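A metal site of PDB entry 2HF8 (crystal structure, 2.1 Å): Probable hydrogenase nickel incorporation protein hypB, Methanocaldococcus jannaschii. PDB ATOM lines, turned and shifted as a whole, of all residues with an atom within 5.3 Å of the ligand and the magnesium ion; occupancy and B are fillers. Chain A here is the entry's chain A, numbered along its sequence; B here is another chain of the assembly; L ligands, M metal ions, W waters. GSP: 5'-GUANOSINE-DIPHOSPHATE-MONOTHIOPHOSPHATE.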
ATOM      1  N   ALA A  46     -14.389  12.092   4.550  1.00  0.00           N
ATOM      2  CA  ALA A  46     -15.761  12.023   5.039  1.00  0.00           C
ATOM      3  C   ALA A  46     -15.777  11.268   6.371  1.00  0.00           C
ATOM      4  O   ALA A  46     -14.725  10.913   6.897  1.00  0.00           O
ATOM      5  CB  ALA A  46     -16.656  11.338   4.003  1.00  0.00           C
ATOM      6  N   ILE A  47     -16.967  11.019   6.909  1.00  0.00           N
ATOM      7  CA  ILE A  47     -17.090  10.297   8.175  1.00  0.00           C
ATOM      8  C   ILE A  47     -16.829   8.810   7.975  1.00  0.00           C
ATOM      9  O   ILE A  47     -17.552   8.159   7.215  1.00  0.00           O
ATOM     10  CB  ILE A  47     -18.487  10.485   8.825  1.00  0.00           C
ATOM     11  CG1 ILE A  47     -18.841  11.963   9.004  1.00  0.00           C
ATOM     12  CG2 ILE A  47     -18.590   9.701  10.145  1.00  0.00           C
ATOM     13  CD1 ILE A  47     -18.141  12.645  10.153  1.00  0.00           C
ATOM     14  N   GLY A  48     -15.807   8.291   8.645  1.00  0.00           N
ATOM     15  CA  GLY A  48     -15.466   6.870   8.592  1.00  0.00           C
ATOM     16  C   GLY A  48     -14.819   6.374   7.308  1.00  0.00           C
ATOM     17  O   GLY A  48     -14.795   5.168   7.052  1.00  0.00           O
ATOM     18  N   SER A  49     -14.297   7.298   6.516  1.00  0.00           N
ATOM     19  CA  SER A  49     -13.575   6.980   5.275  1.00  0.00           C
ATOM     20  C   SER A  49     -12.336   6.100   5.483  1.00  0.00           C
ATOM     21  O   SER A  49     -11.953   5.344   4.583  1.00  0.00           O
ATOM     22  CB  SER A  49     -13.150   8.255   4.558  1.00  0.00           C
ATOM     23  OG  SER A  49     -14.272   8.961   4.064  1.00  0.00           O
ATOM     24  N   GLY A  50     -11.716   6.215   6.653  1.00  0.00           N
ATOM     25  CA  GLY A  50     -10.552   5.407   7.014  1.00  0.00           C
ATOM     26  C   GLY A  50      -9.289   6.187   7.372  1.00  0.00           C
ATOM     27  O   GLY A  50      -8.185   5.633   7.293  1.00  0.00           O
ATOM     28  N   LYS A  51      -9.455   7.441   7.777  1.00  0.00           N
ATOM     29  CA  LYS A  51      -8.329   8.323   8.145  1.00  0.00           C
ATOM     30  C   LYS A  51      -7.457   7.748   9.271  1.00  0.00           C
ATOM     31  O   LYS A  51      -6.236   7.679   9.132  1.00  0.00           O
ATOM     32  CB  LYS A  51      -8.828   9.726   8.557  1.00  0.00           C
ATOM     33  CG  LYS A  51      -9.616  10.490   7.485  1.00  0.00           C
ATOM     34  CD  LYS A  51     -10.101  11.867   7.984  1.00  0.00           C
ATOM     35  CE  LYS A  51     -11.305  11.794   8.929  1.00  0.00           C
ATOM     36  NZ  LYS A  51     -12.398  10.899   8.445  1.00  0.00           N
ATOM     37  N   THR A  52      -8.093   7.337  10.362  1.00  0.00           N
ATOM     38  CA  THR A  52      -7.367   6.778  11.515  1.00  0.00           C
ATOM     39  C   THR A  52      -6.630   5.486  11.155  1.00  0.00           C
ATOM     40  O   THR A  52      -5.443   5.347  11.469  1.00  0.00           O
ATOM     41  CB  THR A  52      -8.294   6.558  12.732  1.00  0.00           C
ATOM     42  OG1 THR A  52      -9.010   7.779  13.014  1.00  0.00           O
ATOM     43  CG2 THR A  52      -7.495   6.162  13.968  1.00  0.00           C
ATOM     44  N   LEU A  53      -7.305   4.573  10.462  1.00  0.00           N
ATOM     45  CA  LEU A  53      -6.697   3.294  10.087  1.00  0.00           C
ATOM     46  C   LEU A  53      -5.514   3.497   9.134  1.00  0.00           C
ATOM     47  O   LEU A  53      -4.523   2.788   9.219  1.00  0.00           O
ATOM     48  CB  LEU A  53      -7.728   2.311   9.490  1.00  0.00           C
ATOM     49  CG  LEU A  53      -7.282   0.858   9.262  1.00  0.00           C
ATOM     50  CD1 LEU A  53      -6.771   0.217  10.554  1.00  0.00           C
ATOM     51  CD2 LEU A  53      -8.405  -0.001   8.652  1.00  0.00           C
ATOM     52  N   LEU A  54      -5.627   4.491   8.245  1.00  0.00           N
ATOM     53  CA  LEU A  54      -4.545   4.832   7.332  1.00  0.00           C
ATOM     54  C   LEU A  54      -3.333   5.345   8.121  1.00  0.00           C
ATOM     55  O   LEU A  54      -2.218   4.900   7.887  1.00  0.00           O
ATOM     56  CB  LEU A  54      -4.993   5.876   6.292  1.00  0.00           C
ATOM     57  CG  LEU A  54      -3.931   6.405   5.314  1.00  0.00           C
ATOM     58  CD1 LEU A  54      -3.273   5.302   4.491  1.00  0.00           C
ATOM     59  CD2 LEU A  54      -4.496   7.514   4.402  1.00  0.00           C
ATOM     60  N   ASP A  74     -11.384  15.951  16.568  1.00  0.00           N
ATOM     61  CA  ASP A  74     -12.768  15.505  16.418  1.00  0.00           C
ATOM     62  C   ASP A  74     -13.621  15.996  17.584  1.00  0.00           C
ATOM     63  O   ASP A  74     -13.097  16.454  18.595  1.00  0.00           O
ATOM     64  CB  ASP A  74     -12.851  13.982  16.315  1.00  0.00           C
ATOM     65  CG  ASP A  74     -14.048  13.494  15.526  1.00  0.00           C
ATOM     66  OD1 ASP A  74     -14.919  14.311  15.123  1.00  0.00           O
ATOM     67  OD2 ASP A  74     -14.141  12.277  15.314  1.00  0.00           O
ATOM     68  N   ASP A  80      -9.836   8.367  18.650  1.00  0.00           N
ATOM     69  CA  ASP A  80      -8.770   8.227  17.676  1.00  0.00           C
ATOM     70  C   ASP A  80      -7.403   8.493  18.279  1.00  0.00           C
ATOM     71  O   ASP A  80      -6.427   7.900  17.849  1.00  0.00           O
ATOM     72  CB  ASP A  80      -9.033   9.122  16.474  1.00  0.00           C
ATOM     73  CG  ASP A  80     -10.203   8.634  15.643  1.00  0.00           C
ATOM     74  OD1 ASP A  80     -10.766   7.560  15.955  1.00  0.00           O
ATOM     75  OD2 ASP A  80     -10.547   9.296  14.646  1.00  0.00           O
ATOM     76  N   ARG A  83      -6.347   5.221  19.737  1.00  0.00           N
ATOM     77  CA  ARG A  83      -5.948   4.321  18.645  1.00  0.00           C
ATOM     78  C   ARG A  83      -4.528   4.577  18.153  1.00  0.00           C
ATOM     79  O   ARG A  83      -3.741   3.637  18.013  1.00  0.00           O
ATOM     80  CB  ARG A  83      -6.957   4.373  17.489  1.00  0.00           C
ATOM     81  CG  ARG A  83      -8.137   3.426  17.696  1.00  0.00           C
ATOM     82  CD  ARG A  83      -9.227   3.604  16.649  1.00  0.00           C
ATOM     83  NE  ARG A  83      -8.810   3.184  15.314  1.00  0.00           N
ATOM     84  CZ  ARG A  83      -9.550   3.302  14.214  1.00  0.00           C
ATOM     85  NH1 ARG A  83     -10.762   3.824  14.271  1.00  0.00           N
ATOM     86  NH2 ARG A  83      -9.061   2.904  13.044  1.00  0.00           N
ATOM     87  N   GLU A 125      -5.020  14.331  11.805  1.00  0.00           N
ATOM     88  CA  GLU A 125      -6.347  13.891  11.397  1.00  0.00           C
ATOM     89  C   GLU A 125      -7.362  14.998  11.624  1.00  0.00           C
ATOM     90  O   GLU A 125      -7.636  15.386  12.759  1.00  0.00           O
ATOM     91  CB  GLU A 125      -6.793  12.594  12.065  1.00  0.00           C
ATOM     92  CG  GLU A 125      -8.064  12.036  11.411  1.00  0.00           C
ATOM     93  CD  GLU A 125      -8.502  10.718  11.996  1.00  0.00           C
ATOM     94  OE1 GLU A 125      -7.632   9.994  12.507  1.00  0.00           O
ATOM     95  OE2 GLU A 125      -9.711  10.405  11.957  1.00  0.00           O
ATOM     96  N   GLY A 128     -14.006  14.711  10.371  1.00  0.00           N
ATOM     97  CA  GLY A 128     -14.723  14.073   9.267  1.00  0.00           C
ATOM     98  C   GLY A 128     -15.747  15.026   8.678  1.00  0.00           C
ATOM     99  O   GLY A 128     -16.766  15.312   9.314  1.00  0.00           O
ATOM    100  N   ASN A 172     -10.650   4.767  -0.782  1.00  0.00           N
ATOM    101  CA  ASN A 172     -10.403   3.656   0.145  1.00  0.00           C
ATOM    102  C   ASN A 172     -11.563   2.662   0.125  1.00  0.00           C
ATOM    103  O   ASN A 172     -12.589   2.909  -0.512  1.00  0.00           O
ATOM    104  CB  ASN A 172     -10.168   4.228   1.559  1.00  0.00           C
ATOM    105  CG  ASN A 172      -9.680   3.176   2.554  1.00  0.00           C
ATOM    106  OD1 ASN A 172     -10.070   3.195   3.727  1.00  0.00           O
ATOM    107  ND2 ASN A 172      -8.834   2.257   2.106  1.00  0.00           N
ATOM    108  N   LYS A 173     -11.385   1.528   0.805  1.00  0.00           N
ATOM    109  CA  LYS A 173     -12.378   0.430   0.871  1.00  0.00           C
ATOM    110  C   LYS A 173     -12.746  -0.092  -0.515  1.00  0.00           C
ATOM    111  O   LYS A 173     -13.923  -0.367  -0.777  1.00  0.00           O
ATOM    112  CB  LYS A 173     -13.646   0.854   1.624  1.00  0.00           C
ATOM    113  CG  LYS A 173     -13.418   1.406   3.018  1.00  0.00           C
ATOM    114  CD  LYS A 173     -14.734   1.710   3.718  1.00  0.00           C
ATOM    115  CE  LYS A 173     -14.533   2.669   4.869  1.00  0.00           C
ATOM    116  NZ  LYS A 173     -15.755   3.514   5.081  1.00  0.00           N
ATOM    117  N   ILE A 174     -11.761  -0.240  -1.389  1.00  0.00           N
ATOM    118  CA  ILE A 174     -12.036  -0.787  -2.717  1.00  0.00           C
ATOM    119  C   ILE A 174     -12.533  -2.235  -2.649  1.00  0.00           C
ATOM    120  O   ILE A 174     -13.204  -2.685  -3.563  1.00  0.00           O
ATOM    121  CB  ILE A 174     -10.844  -0.639  -3.716  1.00  0.00           C
ATOM    122  CG1 ILE A 174      -9.599  -1.389  -3.228  1.00  0.00           C
ATOM    123  CG2 ILE A 174     -10.589   0.851  -4.057  1.00  0.00           C
ATOM    124  CD1 ILE A 174      -8.459  -1.426  -4.253  1.00  0.00           C
ATOM    125  N   ASP A 175     -12.205  -2.921  -1.551  1.00  0.00           N
ATOM    126  CA  ASP A 175     -12.705  -4.283  -1.306  1.00  0.00           C
ATOM    127  C   ASP A 175     -14.230  -4.367  -1.153  1.00  0.00           C
ATOM    128  O   ASP A 175     -14.804  -5.442  -1.304  1.00  0.00           O
ATOM    129  CB  ASP A 175     -12.004  -4.935  -0.096  1.00  0.00           C
ATOM    130  CG  ASP A 175     -12.175  -4.135   1.187  1.00  0.00           C
ATOM    131  OD1 ASP A 175     -11.615  -3.018   1.291  1.00  0.00           O
ATOM    132  OD2 ASP A 175     -12.835  -4.640   2.123  1.00  0.00           O
ATOM    133  N   LEU A 176     -14.865  -3.230  -0.876  1.00  0.00           N
ATOM    134  CA  LEU A 176     -16.317  -3.191  -0.643  1.00  0.00           C
ATOM    135  C   LEU A 176     -17.124  -2.598  -1.804  1.00  0.00           C
ATOM    136  O   LEU A 176     -18.342  -2.423  -1.689  1.00  0.00           O
ATOM    137  CB  LEU A 176     -16.620  -2.401   0.644  1.00  0.00           C
ATOM    138  CG  LEU A 176     -15.927  -2.856   1.928  1.00  0.00           C
ATOM    139  CD1 LEU A 176     -16.324  -1.982   3.090  1.00  0.00           C
ATOM    140  CD2 LEU A 176     -16.223  -4.320   2.225  1.00  0.00           C
ATOM    141  N   LEU A 203      -7.211   2.281  -2.840  1.00  0.00           N
ATOM    142  CA  LEU A 203      -6.706   1.626  -1.639  1.00  0.00           C
ATOM    143  C   LEU A 203      -7.722   0.677  -1.007  1.00  0.00           C
ATOM    144  O   LEU A 203      -8.919   0.940  -1.008  1.00  0.00           O
ATOM    145  CB  LEU A 203      -6.315   2.701  -0.602  1.00  0.00           C
ATOM    146  CG  LEU A 203      -5.703   2.313   0.757  1.00  0.00           C
ATOM    147  CD1 LEU A 203      -4.333   1.651   0.601  1.00  0.00           C
ATOM    148  CD2 LEU A 203      -5.586   3.532   1.673  1.00  0.00           C
ATOM    149  N   SER A 204      -7.212  -0.431  -0.462  1.00  0.00           N
ATOM    150  CA  SER A 204      -7.914  -1.151   0.575  1.00  0.00           C
ATOM    151  C   SER A 204      -6.991  -1.307   1.764  1.00  0.00           C
ATOM    152  O   SER A 204      -5.901  -1.862   1.647  1.00  0.00           O
ATOM    153  CB  SER A 204      -8.397  -2.525   0.103  1.00  0.00           C
ATOM    154  OG  SER A 204      -8.936  -3.254   1.202  1.00  0.00           O
ATOM    155  N   LEU A 205      -7.435  -0.804   2.915  1.00  0.00           N
ATOM    156  CA  LEU A 205      -6.698  -0.978   4.164  1.00  0.00           C
ATOM    157  C   LEU A 205      -6.944  -2.349   4.794  1.00  0.00           C
ATOM    158  O   LEU A 205      -6.258  -2.733   5.741  1.00  0.00           O
ATOM    159  CB  LEU A 205      -7.021   0.165   5.143  1.00  0.00           C
ATOM    160  CG  LEU A 205      -6.430   1.521   4.746  1.00  0.00           C
ATOM    161  CD1 LEU A 205      -7.013   2.660   5.583  1.00  0.00           C
ATOM    162  CD2 LEU A 205      -4.894   1.514   4.818  1.00  0.00           C
ATOM    163  N   LYS A 206      -7.915  -3.078   4.267  1.00  0.00           N
ATOM    164  CA  LYS A 206      -8.156  -4.477   4.653  1.00  0.00           C
ATOM    165  C   LYS A 206      -7.162  -5.421   3.956  1.00  0.00           C
ATOM    166  O   LYS A 206      -6.481  -6.203   4.625  1.00  0.00           O
ATOM    167  CB  LYS A 206      -9.597  -4.871   4.362  1.00  0.00           C
ATOM    168  CG  LYS A 206     -10.017  -6.241   4.891  1.00  0.00           C
ATOM    169  CD  LYS A 206     -11.515  -6.425   4.741  1.00  0.00           C
ATOM    170  CE  LYS A 206     -12.047  -7.608   5.537  1.00  0.00           C
ATOM    171  NZ  LYS A 206     -13.533  -7.708   5.401  1.00  0.00           N
ATOM    172  N   THR B 149     -22.972   1.366   9.180  1.00  0.00           N
ATOM    173  CA  THR B 149     -21.942   0.534   9.807  1.00  0.00           C
ATOM    174  C   THR B 149     -20.559   0.780   9.217  1.00  0.00           C
ATOM    175  O   THR B 149     -19.557   0.665   9.926  1.00  0.00           O
ATOM    176  CB  THR B 149     -22.269  -0.970   9.671  1.00  0.00           C
ATOM    177  OG1 THR B 149     -22.301  -1.344   8.288  1.00  0.00           O
ATOM    178  CG2 THR B 149     -23.600  -1.315  10.339  1.00  0.00           C
ATOM    179  N   THR B 150     -20.514   1.125   7.935  1.00  0.00           N
ATOM    180  CA  THR B 150     -19.253   1.305   7.203  1.00  0.00           C
ATOM    181  C   THR B 150     -18.481   2.566   7.616  1.00  0.00           C
ATOM    182  O   THR B 150     -17.322   2.751   7.239  1.00  0.00           O
ATOM    183  CB  THR B 150     -19.476   1.283   5.663  1.00  0.00           C
ATOM    184  OG1 THR B 150     -20.385   2.316   5.288  1.00  0.00           O
ATOM    185  CG2 THR B 150     -20.023  -0.067   5.219  1.00  0.00           C
ATOM    186  N   GLU B 151     -19.134   3.415   8.401  1.00  0.00           N
ATOM    187  CA  GLU B 151     -18.472   4.561   9.000  1.00  0.00           C
ATOM    188  C   GLU B 151     -17.712   4.173  10.281  1.00  0.00           C
ATOM    189  O   GLU B 151     -16.953   4.975  10.826  1.00  0.00           O
ATOM    190  CB  GLU B 151     -19.498   5.659   9.298  1.00  0.00           C
ATOM    191  CG  GLU B 151     -20.155   6.233   8.037  1.00  0.00           C
ATOM    192  CD  GLU B 151     -21.635   6.547   8.232  1.00  0.00           C
ATOM    193  OE1 GLU B 151     -22.064   6.807   9.375  1.00  0.00           O
ATOM    194  OE2 GLU B 151     -22.373   6.514   7.222  1.00  0.00           O
ATOM    195  N   GLY B 152     -17.891   2.935  10.752  1.00  0.00           N
ATOM    196  CA  GLY B 152     -17.254   2.482  11.992  1.00  0.00           C
ATOM    197  C   GLY B 152     -18.231   2.492  13.149  1.00  0.00           C
ATOM    198  O   GLY B 152     -19.152   3.299  13.174  1.00  0.00           O
ATOM    199  N   ASP B 153     -18.031   1.603  14.126  1.00  0.00           N
ATOM    200  CA  ASP B 153     -18.995   1.447  15.220  1.00  0.00           C
ATOM    201  C   ASP B 153     -18.820   2.430  16.376  1.00  0.00           C
ATOM    202  O   ASP B 153     -19.545   2.358  17.369  1.00  0.00           O
ATOM    203  CB  ASP B 153     -19.097  -0.022  15.707  1.00  0.00           C
ATOM    204  CG  ASP B 153     -17.782  -0.582  16.210  1.00  0.00           C
ATOM    205  OD1 ASP B 153     -16.885   0.192  16.617  1.00  0.00           O
ATOM    206  OD2 ASP B 153     -17.640  -1.837  16.211  1.00  0.00           O
ATOM    207  N   THR B 155     -19.071   5.693  15.555  1.00  0.00           N
ATOM    208  CA  THR B 155     -19.698   6.874  14.937  1.00  0.00           C
ATOM    209  C   THR B 155     -20.808   7.500  15.787  1.00  0.00           C
ATOM    210  O   THR B 155     -20.926   8.722  15.862  1.00  0.00           O
ATOM    211  CB  THR B 155     -20.239   6.542  13.512  1.00  0.00           C
ATOM    212  OG1 THR B 155     -19.157   6.093  12.687  1.00  0.00           O
ATOM    213  CG2 THR B 155     -20.869   7.767  12.857  1.00  0.00           C
ATOM    214  N   LYS B 158     -19.289   9.040  19.021  1.00  0.00           N
ATOM    215  CA  LYS B 158     -18.464  10.175  18.583  1.00  0.00           C
ATOM    216  C   LYS B 158     -19.277  11.439  18.283  1.00  0.00           C
ATOM    217  O   LYS B 158     -18.708  12.534  18.194  1.00  0.00           O
ATOM    218  CB  LYS B 158     -17.661   9.815  17.330  1.00  0.00           C
ATOM    219  CG  LYS B 158     -16.387   9.022  17.580  1.00  0.00           C
ATOM    220  CD  LYS B 158     -15.660   8.784  16.264  1.00  0.00           C
ATOM    221  CE  LYS B 158     -14.453   7.899  16.445  1.00  0.00           C
ATOM    222  NZ  LYS B 158     -13.718   7.765  15.145  1.00  0.00           N
ATOM    223  N   HIS B 159     -20.588  11.289  18.115  1.00  0.00           N
ATOM    224  CA  HIS B 159     -21.439  12.427  17.751  1.00  0.00           C
ATOM    225  C   HIS B 159     -22.721  12.510  18.584  1.00  0.00           C
ATOM    226  O   HIS B 159     -23.824  12.496  18.019  1.00  0.00           O
ATOM    227  CB  HIS B 159     -21.776  12.385  16.253  1.00  0.00           C
ATOM    228  CG  HIS B 159     -20.582  12.256  15.356  1.00  0.00           C
ATOM    229  ND1 HIS B 159     -20.127  11.031  14.911  1.00  0.00           N
ATOM    230  CD2 HIS B 159     -19.746  13.184  14.843  1.00  0.00           C
ATOM    231  CE1 HIS B 159     -19.067  11.220  14.152  1.00  0.00           C
ATOM    232  NE2 HIS B 159     -18.813  12.519  14.090  1.00  0.00           N
ATOM    233  N   ALA B 179     -17.875  -6.942   7.242  1.00  0.00           N
ATOM    234  CA  ALA B 179     -16.811  -6.531   6.316  1.00  0.00           C
ATOM    235  C   ALA B 179     -15.927  -5.390   6.840  1.00  0.00           C
ATOM    236  O   ALA B 179     -14.728  -5.346   6.539  1.00  0.00           O
ATOM    237  CB  ALA B 179     -17.419  -6.154   4.966  1.00  0.00           C
ATOM    238  N   VAL B 180     -16.516  -4.473   7.612  1.00  0.00           N
ATOM    239  CA  VAL B 180     -15.766  -3.348   8.210  1.00  0.00           C
ATOM    240  C   VAL B 180     -15.387  -3.582   9.675  1.00  0.00           C
ATOM    241  O   VAL B 180     -14.740  -2.751  10.305  1.00  0.00           O
ATOM    242  CB  VAL B 180     -16.531  -1.997   8.082  1.00  0.00           C
ATOM    243  CG1 VAL B 180     -16.538  -1.495   6.645  1.00  0.00           C
ATOM    244  CG2 VAL B 180     -17.948  -2.113   8.634  1.00  0.00           C
ATOM    245  N   GLY B 181     -15.807  -4.727  10.219  1.00  0.00           N
ATOM    246  CA  GLY B 181     -15.548  -5.045  11.621  1.00  0.00           C
ATOM    247  C   GLY B 181     -16.436  -4.299  12.616  1.00  0.00           C
ATOM    248  O   GLY B 181     -16.076  -4.172  13.795  1.00  0.00           O
ATOM    249  N   ALA B 182     -17.591  -3.830  12.159  1.00  0.00           N
ATOM    250  CA  ALA B 182     -18.533  -3.085  13.019  1.00  0.00           C
ATOM    251  C   ALA B 182     -19.414  -3.992  13.872  1.00  0.00           C
ATOM    252  O   ALA B 182     -19.981  -4.973  13.384  1.00  0.00           O
ATOM    253  CB  ALA B 182     -19.390  -2.152  12.178  1.00  0.00           C
HETATM  254  PG  GSP L   1     -13.743   9.134  11.751  1.00  0.00           P
HETATM  255  O3B GSP L   1     -13.470   7.838  10.847  1.00  0.00           O
HETATM  256  S1G GSP L   1     -14.372  10.407  10.797  1.00  0.00           S
HETATM  257  O2G GSP L   1     -14.809   8.741  12.810  1.00  0.00           O
HETATM  258  O3G GSP L   1     -12.449   9.603  12.426  1.00  0.00           O
HETATM  259  PB  GSP L   1     -12.110   7.489  10.059  1.00  0.00           P
HETATM  260  O1B GSP L   1     -12.079   8.193   8.762  1.00  0.00           O
HETATM  261  O2B GSP L   1     -10.892   7.765  10.861  1.00  0.00           O
HETATM  262  PA  GSP L   1     -11.713   4.711  10.574  1.00  0.00           P
HETATM  263  O1A GSP L   1     -10.240   4.576  10.423  1.00  0.00           O
HETATM  264  O2A GSP L   1     -12.125   4.836  11.989  1.00  0.00           O
HETATM  265  O3A GSP L   1     -12.289   5.935   9.722  1.00  0.00           O
HETATM  266  O5' GSP L   1     -12.422   3.485   9.824  1.00  0.00           O
HETATM  267  C5' GSP L   1     -13.826   3.376   9.769  1.00  0.00           C
HETATM  268  C4' GSP L   1     -14.216   1.903   9.592  1.00  0.00           C
HETATM  269  O4' GSP L   1     -13.870   1.453   8.304  1.00  0.00           O
HETATM  270  C3' GSP L   1     -13.501   0.968  10.560  1.00  0.00           C
HETATM  271  O3' GSP L   1     -14.468  -0.004  10.893  1.00  0.00           O
HETATM  272  C2' GSP L   1     -12.391   0.350   9.730  1.00  0.00           C
HETATM  273  O2' GSP L   1     -12.054  -0.951  10.150  1.00  0.00           O
HETATM  274  C1' GSP L   1     -13.033   0.299   8.366  1.00  0.00           C
HETATM  275  N9  GSP L   1     -12.141   0.383   7.204  1.00  0.00           N
HETATM  276  C8  GSP L   1     -11.251   1.386   6.902  1.00  0.00           C
HETATM  277  N7  GSP L   1     -10.683   1.080   5.709  1.00  0.00           N
HETATM  278  C5  GSP L   1     -11.217  -0.070   5.247  1.00  0.00           C
HETATM  279  C6  GSP L   1     -11.017  -0.813   4.086  1.00  0.00           C
HETATM  280  O6  GSP L   1     -10.194  -0.435   3.254  1.00  0.00           O
HETATM  281  N1  GSP L   1     -11.728  -1.986   3.884  1.00  0.00           N
HETATM  282  C2  GSP L   1     -12.645  -2.406   4.824  1.00  0.00           C
HETATM  283  N2  GSP L   1     -13.338  -3.523   4.623  1.00  0.00           N
HETATM  284  N3  GSP L   1     -12.845  -1.671   5.964  1.00  0.00           N
HETATM  285  C4  GSP L   1     -12.148  -0.522   6.176  1.00  0.00           C
HETATM  286 MG    MG M   1     -10.735   8.761  12.725  1.00  0.00          MG
HETATM  287  O   HOH W   1     -11.427  -3.359   8.447  1.00  0.00           O
HETATM  288  O   HOH W   2     -11.617   7.079  13.486  1.00  0.00           O
HETATM  289  O   HOH W   3     -15.869  -0.303  13.336  1.00  0.00           O
HETATM  290  O   HOH W   4     -17.523   8.574  13.047  1.00  0.00           O
HETATM  291  O   HOH W   5     -15.920  11.375  13.553  1.00  0.00           O
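An oxygen (O1A) of the ligand sits at hydrogen-bond distance from the backbone NH (N) of Thr 52 (3.5 Å).
N of Lys 51 lies within hydrogen-bond range of O1B of the ligand.
O1B of the ligand lies within salt-bridge range of NZ of Lys 51.
The side-chain amino group of Lys 158 of chain B lies within hydrogen-bond range of an oxygen (O2G) of the ligand, 2.8 Å away.
OD2 of Asp 175 is in hydrogen-bond range of N2 of the ligand (2.8 Å).
N of Leu 205 lies within hydrogen-bond range of O6 of the ligand, at 2.8 Å.
O3' of the ligand lies within hydrogen-bond range of O of Val 180 of chain B (2.8 Å).
An oxygen (O2A) of the ligand lies within salt-bridge range of the guanidinium group (NH1) of Arg 83, 2.8 Å away.
An oxygen (O1B) of the ligand sits at hydrogen-bond distance from the backbone NH of Gly 50 (2.9 Å).
N of Leu 53 lies within hydrogen-bond range of O1A of the ligand, 2.9 Å away.
N7 of the ligand sits close to OD1 of Asn 172.
A nitrogen (N2) of the ligand sits at hydrogen-bond distance from the backbone carbonyl oxygen (O) of Ala 179 of chain B, 3.0 Å away.
N of Gly 48 lies close to O3B of the ligand, 3.2 Å away.
The backbone NH (N) of Ser 49 sits at hydrogen-bond distance from an oxygen (O1B) of the ligand (3.3 Å).
The backbone NH (N) of Lys 173 sits close to an oxygen (O6) of the ligand (3.4 Å).
OD1 of Asp 80 lies within salt-bridge range of NZ of Lys 158 of chain B (3.1 Å).
OG of Ser 204 sits at hydrogen-bond distance from OD1 of Asp 175 (2.7 Å).
The backbone NH (N) of Leu 205 lies close to the side-chain amide nitrogen (ND2) of Asn 172 (3.5 Å).
OD1 of Asn 172 sits close to O of Ser 49.
The side-chain amide nitrogen of Asn 172 lies close to the backbone carbonyl oxygen of Leu 203 (3.4 Å).
O of Ala 179 of chain B is in hydrogen-bond range of NZ of Lys 206 (2.9 Å).
O of Gly 48 lies within hydrogen-bond range of NZ of Lys 173.
O of Glu 151 of chain B is in hydrogen-bond range of OG1 of Thr 155 of chain B (3.1 Å).
Ala 46 touches the ligand (O to S1G, 3.9 Å).
Ile 47 touches the ligand (CA to S1G, 3.8 Å).
Gly 128 touches the ligand (CA to S1G, 3.99 Å).
Leu 176 touches the ligand (CD1 to N2, 3.7 Å).
CA of Ser 204 touches O6 of the ligand, 3.6 Å away.
Lys 206 touches the ligand.
O of Thr 150 of chain B touches O4' of the ligand (3.8 Å).
O of Glu 151 of chain B touches C5' of the ligand, at 3.7 Å.
CA of Gly 152 of chain B touches O3' of the ligand, 3.9 Å away.
Hydrophobic or aromatic side chains that line the ligand: Leu 53, Leu 176, Leu 205 and Val 180 of chain B.
Of the 35 residues printed, 25 come within 4 Å of the ligand.
Merely in contact with the magnesium ion: Lys 158 of chain B (3.97 Å).
The magnesium ion is bound by O3G of the ligand, at 1.9 Å.
The magnesium ion is bound by OD2 of Asp 80 (2.0 Å).
OG1 of Thr 52 binds the magnesium ion, at 2.0 Å.
The magnesium ion is bound by water W2.
OE2 of Glu 125 binds the magnesium ion (2.1 Å).
The magnesium ion is bound by O2B of the ligand, 2.1 Å away.
The magnesium ion has six donor atoms within binding distance.
Water W2 lies within hydrogen-bond range of the side-chain carboxylate of Asp 80 (2.7 Å), an oxygen (O2A) of the ligand (2.7 Å), the side-chain amino group of Lys 158 of chain B (2.8 Å) and the guanidinium group of Arg 83 (3.5 Å).
Water W4 bridges O2G of the ligand (2.7 Å) and OG1 of Thr 155 of chain B (3.0 Å).
Water W3 bridges O3' of the ligand (2.8 Å) and N of Asp 153 of chain B (3.0 Å).
Water W5 lies within hydrogen-bond range of the side-chain carboxylate (OD2) of Asp 74 (2.7 Å), an oxygen (O2G) of the ligand (3.0 Å) and a ring nitrogen (NE2) of His 159 of chain B (3.2 Å).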
